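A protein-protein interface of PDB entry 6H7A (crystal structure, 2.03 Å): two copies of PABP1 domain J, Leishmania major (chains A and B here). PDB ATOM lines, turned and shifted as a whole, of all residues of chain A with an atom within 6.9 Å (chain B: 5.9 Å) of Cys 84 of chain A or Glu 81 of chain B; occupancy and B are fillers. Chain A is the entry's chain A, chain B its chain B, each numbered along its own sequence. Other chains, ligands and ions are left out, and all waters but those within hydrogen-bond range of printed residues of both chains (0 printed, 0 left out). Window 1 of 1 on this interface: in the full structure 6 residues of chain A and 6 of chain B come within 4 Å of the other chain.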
ATOM      1  N   ARG A  78      14.193  -5.681 -27.711  1.00  0.00           N
ATOM      2  CA  ARG A  78      14.719  -6.799 -26.933  1.00  0.00           C
ATOM      3  C   ARG A  78      15.808  -6.349 -25.968  1.00  0.00           C
ATOM      4  O   ARG A  78      15.930  -6.909 -24.872  1.00  0.00           O
ATOM      5  CB  ARG A  78      15.259  -7.888 -27.860  1.00  0.00           C
ATOM      6  CG  ARG A  78      14.245  -8.442 -28.853  1.00  0.00           C
ATOM      7  CD  ARG A  78      12.949  -8.850 -28.178  1.00  0.00           C
ATOM      8  NE  ARG A  78      13.116 -10.011 -27.311  1.00  0.00           N
ATOM      9  CZ  ARG A  78      12.109 -10.659 -26.733  1.00  0.00           C
ATOM     10  NH1 ARG A  78      10.861 -10.257 -26.931  1.00  0.00           N
ATOM     11  NH2 ARG A  78      12.348 -11.708 -25.958  1.00  0.00           N
ATOM     12  N   VAL A  79      16.606  -5.351 -26.350  1.00  0.00           N
ATOM     13  CA  VAL A  79      17.635  -4.842 -25.447  1.00  0.00           C
ATOM     14  C   VAL A  79      16.996  -4.165 -24.243  1.00  0.00           C
ATOM     15  O   VAL A  79      17.398  -4.392 -23.096  1.00  0.00           O
ATOM     16  CB  VAL A  79      18.589  -3.890 -26.193  1.00  0.00           C
ATOM     17  CG1 VAL A  79      19.518  -3.188 -25.211  1.00  0.00           C
ATOM     18  CG2 VAL A  79      19.396  -4.654 -27.232  1.00  0.00           C
ATOM     19  N   THR A  80      15.987  -3.324 -24.486  1.00  0.00           N
ATOM     20  CA  THR A  80      15.257  -2.704 -23.384  1.00  0.00           C
ATOM     21  C   THR A  80      14.608  -3.759 -22.497  1.00  0.00           C
ATOM     22  O   THR A  80      14.644  -3.654 -21.264  1.00  0.00           O
ATOM     23  CB  THR A  80      14.204  -1.737 -23.929  1.00  0.00           C
ATOM     24  OG1 THR A  80      14.852  -0.658 -24.615  1.00  0.00           O
ATOM     25  CG2 THR A  80      13.352  -1.174 -22.800  1.00  0.00           C
ATOM     26  N   GLU A  81      14.019  -4.791 -23.107  1.00  0.00           N
ATOM     27  CA  GLU A  81      13.437  -5.878 -22.327  1.00  0.00           C
ATOM     28  C   GLU A  81      14.506  -6.627 -21.542  1.00  0.00           C
ATOM     29  O   GLU A  81      14.297  -6.976 -20.373  1.00  0.00           O
ATOM     30  CB  GLU A  81      12.676  -6.833 -23.246  1.00  0.00           C
ATOM     31  CG  GLU A  81      12.069  -8.030 -22.535  1.00  0.00           C
ATOM     32  CD  GLU A  81      11.287  -8.929 -23.472  1.00  0.00           C
ATOM     33  OE1 GLU A  81      11.168  -8.583 -24.667  1.00  0.00           O
ATOM     34  OE2 GLU A  81      10.792  -9.981 -23.015  1.00  0.00           O
ATOM     35  N   ALA A  82      15.660  -6.879 -22.165  1.00  0.00           N
ATOM     36  CA  ALA A  82      16.743  -7.563 -21.465  1.00  0.00           C
ATOM     37  C   ALA A  82      17.281  -6.720 -20.317  1.00  0.00           C
ATOM     38  O   ALA A  82      17.591  -7.249 -19.243  1.00  0.00           O
ATOM     39  CB  ALA A  82      17.864  -7.915 -22.443  1.00  0.00           C
ATOM     40  N   LEU A  83      17.398  -5.405 -20.522  1.00  0.00           N
ATOM     41  CA  LEU A  83      17.841  -4.522 -19.447  1.00  0.00           C
ATOM     42  C   LEU A  83      16.858  -4.531 -18.286  1.00  0.00           C
ATOM     43  O   LEU A  83      17.259  -4.444 -17.119  1.00  0.00           O
ATOM     44  CB  LEU A  83      18.027  -3.100 -19.976  1.00  0.00           C
ATOM     45  CG  LEU A  83      19.282  -2.816 -20.802  1.00  0.00           C
ATOM     46  CD1 LEU A  83      19.215  -1.426 -21.411  1.00  0.00           C
ATOM     47  CD2 LEU A  83      20.519  -2.961 -19.938  1.00  0.00           C
ATOM     48  N   CYS A  84      15.562  -4.637 -18.585  1.00  0.00           N
ATOM     49  CA  CYS A  84      14.554  -4.663 -17.533  1.00  0.00           C
ATOM     50  C   CYS A  84      14.519  -6.000 -16.805  1.00  0.00           C
ATOM     51  O   CYS A  84      14.184  -6.043 -15.616  1.00  0.00           O
ATOM     52  CB  CYS A  84      13.184  -4.335 -18.119  1.00  0.00           C
ATOM     53  SG  CYS A  84      13.013  -2.600 -18.587  1.00  0.00           S
ATOM     54  N   VAL A  85      14.862  -7.092 -17.491  1.00  0.00           N
ATOM     55  CA  VAL A  85      15.015  -8.373 -16.805  1.00  0.00           C
ATOM     56  C   VAL A  85      16.174  -8.305 -15.820  1.00  0.00           C
ATOM     57  O   VAL A  85      16.087  -8.816 -14.696  1.00  0.00           O
ATOM     58  CB  VAL A  85      15.202  -9.510 -17.828  1.00  0.00           C
ATOM     59  CG1 VAL A  85      15.581 -10.810 -17.130  1.00  0.00           C
ATOM     60  CG2 VAL A  85      13.935  -9.700 -18.651  1.00  0.00           C
ATOM     61  N   LEU A  86      17.272  -7.658 -16.219  1.00  0.00           N
ATOM     62  CA  LEU A  86      18.419  -7.523 -15.326  1.00  0.00           C
ATOM     63  C   LEU A  86      18.086  -6.647 -14.124  1.00  0.00           C
ATOM     64  O   LEU A  86      18.555  -6.911 -13.010  1.00  0.00           O
ATOM     65  CB  LEU A  86      19.615  -6.958 -16.093  1.00  0.00           C
ATOM     66  CG  LEU A  86      20.173  -7.876 -17.182  1.00  0.00           C
ATOM     67  CD1 LEU A  86      21.362  -7.235 -17.880  1.00  0.00           C
ATOM     68  CD2 LEU A  86      20.551  -9.223 -16.591  1.00  0.00           C
ATOM     69  N   LYS A  87      17.279  -5.602 -14.326  1.00  0.00           N
ATOM     70  CA  LYS A  87      16.864  -4.770 -13.202  1.00  0.00           C
ATOM     71  C   LYS A  87      15.960  -5.535 -12.245  1.00  0.00           C
ATOM     72  O   LYS A  87      16.025  -5.325 -11.029  1.00  0.00           O
ATOM     73  CB  LYS A  87      16.161  -3.508 -13.708  1.00  0.00           C
ATOM     74  CG  LYS A  87      15.729  -2.557 -12.602  1.00  0.00           C
ATOM     75  CD  LYS A  87      15.066  -1.310 -13.162  1.00  0.00           C
ATOM     76  CE  LYS A  87      14.657  -0.358 -12.048  1.00  0.00           C
ATOM     77  NZ  LYS A  87      14.062   0.901 -12.578  1.00  0.00           N
ATOM     78  N   ALA A  88      15.116  -6.425 -12.770  1.00  0.00           N
ATOM     79  CA  ALA A  88      14.237  -7.214 -11.916  1.00  0.00           C
ATOM     80  C   ALA A  88      14.996  -8.246 -11.094  1.00  0.00           C
ATOM     81  O   ALA A  88      14.474  -8.713 -10.076  1.00  0.00           O
ATOM     82  CB  ALA A  88      13.165  -7.907 -12.760  1.00  0.00           C
ATOM     83  N   HIS A  89      16.210  -8.608 -11.504  1.00  0.00           N
ATOM     84  CA  HIS A  89      17.023  -9.582 -10.790  1.00  0.00           C
ATOM     85  C   HIS A  89      17.884  -8.952  -9.701  1.00  0.00           C
ATOM     86  O   HIS A  89      18.741  -9.638  -9.135  1.00  0.00           O
ATOM     87  CB  HIS A  89      17.915 -10.347 -11.772  1.00  0.00           C
ATOM     88  CG  HIS A  89      17.161 -11.254 -12.695  1.00  0.00           C
ATOM     89  ND1 HIS A  89      17.790 -12.075 -13.606  1.00  0.00           N
ATOM     90  CD2 HIS A  89      15.834 -11.470 -12.846  1.00  0.00           C
ATOM     91  CE1 HIS A  89      16.881 -12.758 -14.280  1.00  0.00           C
ATOM     92  NE2 HIS A  89      15.686 -12.409 -13.838  1.00  0.00           N
ATOM     93  N   GLU B  76       6.299 -11.740  -9.883  1.00  0.00           N
ATOM     94  CA  GLU B  76       6.828 -10.462  -9.417  1.00  0.00           C
ATOM     95  C   GLU B  76       7.861  -9.904 -10.388  1.00  0.00           C
ATOM     96  O   GLU B  76       7.875  -8.699 -10.667  1.00  0.00           O
ATOM     97  CB  GLU B  76       7.439 -10.617  -8.025  1.00  0.00           C
ATOM     98  CG  GLU B  76       6.455 -11.008  -6.935  1.00  0.00           C
ATOM     99  CD  GLU B  76       7.125 -11.147  -5.582  1.00  0.00           C
ATOM    100  OE1 GLU B  76       8.369 -11.038  -5.523  1.00  0.00           O
ATOM    101  OE2 GLU B  76       6.413 -11.360  -4.579  1.00  0.00           O
ATOM    102  N   GLU B  77       8.737 -10.764 -10.915  1.00  0.00           N
ATOM    103  CA  GLU B  77       9.768 -10.295 -11.838  1.00  0.00           C
ATOM    104  C   GLU B  77       9.164  -9.809 -13.149  1.00  0.00           C
ATOM    105  O   GLU B  77       9.642  -8.827 -13.729  1.00  0.00           O
ATOM    106  CB  GLU B  77      10.789 -11.399 -12.102  1.00  0.00           C
ATOM    107  CG  GLU B  77      11.718 -11.659 -10.935  1.00  0.00           C
ATOM    108  CD  GLU B  77      12.652 -12.822 -11.188  1.00  0.00           C
ATOM    109  OE1 GLU B  77      12.189 -13.848 -11.728  1.00  0.00           O
ATOM    110  OE2 GLU B  77      13.847 -12.707 -10.849  1.00  0.00           O
ATOM    111  N   ARG B  78       8.122 -10.484 -13.637  1.00  0.00           N
ATOM    112  CA  ARG B  78       7.476 -10.036 -14.865  1.00  0.00           C
ATOM    113  C   ARG B  78       6.767  -8.704 -14.668  1.00  0.00           C
ATOM    114  O   ARG B  78       6.738  -7.877 -15.587  1.00  0.00           O
ATOM    115  CB  ARG B  78       6.491 -11.094 -15.362  1.00  0.00           C
ATOM    116  CG  ARG B  78       7.144 -12.399 -15.791  1.00  0.00           C
ATOM    117  CD  ARG B  78       8.068 -12.200 -16.980  1.00  0.00           C
ATOM    118  NE  ARG B  78       8.747 -13.439 -17.347  1.00  0.00           N
ATOM    119  CZ  ARG B  78       8.227 -14.369 -18.140  1.00  0.00           C
ATOM    120  NH1 ARG B  78       7.017 -14.205 -18.656  1.00  0.00           N
ATOM    121  NH2 ARG B  78       8.917 -15.468 -18.416  1.00  0.00           N
ATOM    122  N   VAL B  79       6.198  -8.474 -13.483  1.00  0.00           N
ATOM    123  CA  VAL B  79       5.580  -7.183 -13.200  1.00  0.00           C
ATOM    124  C   VAL B  79       6.644  -6.099 -13.084  1.00  0.00           C
ATOM    125  O   VAL B  79       6.491  -4.998 -13.627  1.00  0.00           O
ATOM    126  CB  VAL B  79       4.715  -7.269 -11.929  1.00  0.00           C
ATOM    127  CG1 VAL B  79       4.232  -5.886 -11.518  1.00  0.00           C
ATOM    128  CG2 VAL B  79       3.533  -8.201 -12.154  1.00  0.00           C
ATOM    129  N   THR B  80       7.738  -6.391 -12.376  1.00  0.00           N
ATOM    130  CA  THR B  80       8.843  -5.441 -12.295  1.00  0.00           C
ATOM    131  C   THR B  80       9.430  -5.167 -13.673  1.00  0.00           C
ATOM    132  O   THR B  80       9.762  -4.021 -14.001  1.00  0.00           O
ATOM    133  CB  THR B  80       9.920  -5.969 -11.346  1.00  0.00           C
ATOM    134  OG1 THR B  80       9.371  -6.117 -10.031  1.00  0.00           O
ATOM    135  CG2 THR B  80      11.104  -5.013 -11.292  1.00  0.00           C
ATOM    136  N   GLU B  81       9.558  -6.208 -14.500  1.00  0.00           N
ATOM    137  CA  GLU B  81      10.029  -6.016 -15.867  1.00  0.00           C
ATOM    138  C   GLU B  81       9.071  -5.140 -16.663  1.00  0.00           C
ATOM    139  O   GLU B  81       9.503  -4.246 -17.399  1.00  0.00           O
ATOM    140  CB  GLU B  81      10.211  -7.371 -16.550  1.00  0.00           C
ATOM    141  CG  GLU B  81      10.462  -7.289 -18.045  1.00  0.00           C
ATOM    142  CD  GLU B  81      10.400  -8.646 -18.719  1.00  0.00           C
ATOM    143  OE1 GLU B  81      10.511  -9.669 -18.011  1.00  0.00           O
ATOM    144  OE2 GLU B  81      10.234  -8.691 -19.955  1.00  0.00           O
ATOM    145  N   ALA B  82       7.764  -5.380 -16.525  1.00  0.00           N
ATOM    146  CA  ALA B  82       6.783  -4.590 -17.263  1.00  0.00           C
ATOM    147  C   ALA B  82       6.803  -3.131 -16.824  1.00  0.00           C
ATOM    148  O   ALA B  82       6.683  -2.224 -17.656  1.00  0.00           O
ATOM    149  CB  ALA B  82       5.387  -5.186 -17.086  1.00  0.00           C
ATOM    150  N   LEU B  83       6.949  -2.885 -15.519  1.00  0.00           N
ATOM    151  CA  LEU B  83       7.037  -1.511 -15.033  1.00  0.00           C
ATOM    152  C   LEU B  83       8.284  -0.819 -15.567  1.00  0.00           C
ATOM    153  O   LEU B  83       8.248   0.369 -15.908  1.00  0.00           O
ATOM    154  CB  LEU B  83       7.028  -1.494 -13.504  1.00  0.00           C
ATOM    155  CG  LEU B  83       5.711  -1.863 -12.820  1.00  0.00           C
ATOM    156  CD1 LEU B  83       5.903  -1.983 -11.317  1.00  0.00           C
ATOM    157  CD2 LEU B  83       4.643  -0.833 -13.142  1.00  0.00           C
ATOM    158  N   CYS B  84       9.397  -1.550 -15.650  1.00  0.00           N
ATOM    159  CA  CYS B  84      10.634  -0.970 -16.158  1.00  0.00           C
ATOM    160  C   CYS B  84      10.525  -0.640 -17.643  1.00  0.00           C
ATOM    161  O   CYS B  84      11.044   0.388 -18.094  1.00  0.00           O
ATOM    162  CB  CYS B  84      11.797  -1.928 -15.897  1.00  0.00           C
ATOM    163  SG  CYS B  84      13.305  -1.603 -16.839  1.00  0.00           S
ATOM    164  N   VAL B  85       9.860  -1.500 -18.416  1.00  0.00           N
ATOM    165  CA  VAL B  85       9.679  -1.229 -19.839  1.00  0.00           C
ATOM    166  C   VAL B  85       8.812   0.007 -20.039  1.00  0.00           C
ATOM    167  O   VAL B  85       9.108   0.861 -20.884  1.00  0.00           O
ATOM    168  CB  VAL B  85       9.088  -2.461 -20.549  1.00  0.00           C
ATOM    169  CG1 VAL B  85       8.718  -2.125 -21.985  1.00  0.00           C
ATOM    170  CG2 VAL B  85      10.077  -3.615 -20.515  1.00  0.00           C
ATOM    171  N   LEU B  86       7.733   0.129 -19.261  1.00  0.00           N
ATOM    172  CA  LEU B  86       6.900   1.324 -19.336  1.00  0.00           C
ATOM    173  C   LEU B  86       7.676   2.561 -18.903  1.00  0.00           C
ATOM    174  O   LEU B  86       7.537   3.632 -19.504  1.00  0.00           O
ATOM    175  CB  LEU B  86       5.647   1.147 -18.478  1.00  0.00           C
ATOM    176  CG  LEU B  86       4.663   0.067 -18.932  1.00  0.00           C
ATOM    177  CD1 LEU B  86       3.514  -0.061 -17.948  1.00  0.00           C
ATOM    178  CD2 LEU B  86       4.144   0.375 -20.329  1.00  0.00           C
ATOM    179  N   ALA B  88      10.901   2.941 -19.184  1.00  0.00           N
ATOM    180  CA  ALA B  88      11.894   3.224 -20.214  1.00  0.00           C
ATOM    181  C   ALA B  88      11.324   4.103 -21.319  1.00  0.00           C
ATOM    182  O   ALA B  88      12.041   4.938 -21.880  1.00  0.00           O
ATOM    183  CB  ALA B  88      12.431   1.917 -20.799  1.00  0.00           C
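Printed residues of chain B within 4 Å of Glu 81 of chain A: Glu 81 (3.2 Å). Of chain B, only Glu 81, Cys 84 and Val 85 come within 4 Å of Cys 84 of chain A. Printed residues of chain B within 4 Å of Val 85 of chain A: Glu 81. Of the printed residues of chain B, Ala 88 of chain A touches Glu 77 (3.8 Å) and Thr 80 (3.8 Å). Of the printed residues of chain A, Glu 77 of chain B touches Ala 88 and His 89. Of the printed residues of chain A, Thr 80 of chain B touches Ala 88. Of chain A, only Glu 81 (3.2 Å), Cys 84 (3.8 Å) and Val 85 (3.5 Å) come within 4 Å of Glu 81 of chain B.
The side-chain carboxylate (OE2) of Glu 81 of chain A lies close to the side-chain carboxylate (OE2) of Glu 81 of chain B (3.4 Å). SG of Cys 84 of chain A is disulfide-bonded to SG of Cys 84 of chain B. The side-chain sulfur (SG) of Cys 84 of chain A sits at hydrogen-bond distance from the backbone NH (N) of Val 85 of chain B (3.3 Å).
Ala 88 of chain B touches Thr 80 of chain A. O of Glu 81 of chain B touches CB of Cys 84 of chain A (3.8 Å). CG2 of Val 85 of chain A touches OE1 of Glu 81 of chain B (3.5 Å). Ala 88 of chain A touches Glu 77 of chain B (CB to O, 3.8 Å). Thr 80 of chain B touches Ala 88 of chain A. His 89 of chain A touches Glu 77 of chain B.
The side-chain hydroxyl of Thr 80 of chain B is in hydrogen-bond range of the backbone carbonyl oxygen of Glu 76 of chain B, at 3.1 Å. The guanidinium group of Arg 78 of chain A lies within salt-bridge range of the side-chain carboxylate of Glu 81 of chain A, at 2.8 Å.
Printed residues of chain B that touch a printed residue of chain A: Glu 77, Thr 80, Glu 81, Cys 84, Val 85 and Ala 88. Hydrophobic or aromatic side chains of chain B within 4 Å of the printed part of chain A: Val 85 and Ala 88. Along chain B the printed residues that touch a printed residue of chain A span positions 77 to 88. Printed residues of chain A that touch a printed residue of chain B: Thr 80, Glu 81, Cys 84, Val 85, Ala 88 and His 89. Hydrophobic or aromatic side chains of chain A that line the printed part of chain B: Val 85, Ala 88 and His 89.
Thr 80 of chain A touches Ala 88 of chain B, and with the chains exchanged Ala 88 of chain A touches Thr 80 of chain B. Cys 84 of chain A touches Glu 81 of chain B, but with the chains exchanged Glu 81 of chain A does not touch Cys 84 of chain B (6.5 Å). Cys 84 of chain B touches its own counterpart, Cys 84 of chain A. Cys 84 of chain A touches Val 85 of chain B, but with the chains exchanged Val 85 of chain A does not touch Cys 84 of chain B (5.7 Å). Positions printed for both chains: 78, 79, 80, 81, 82, 83, 84, 85, 86 and 88.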
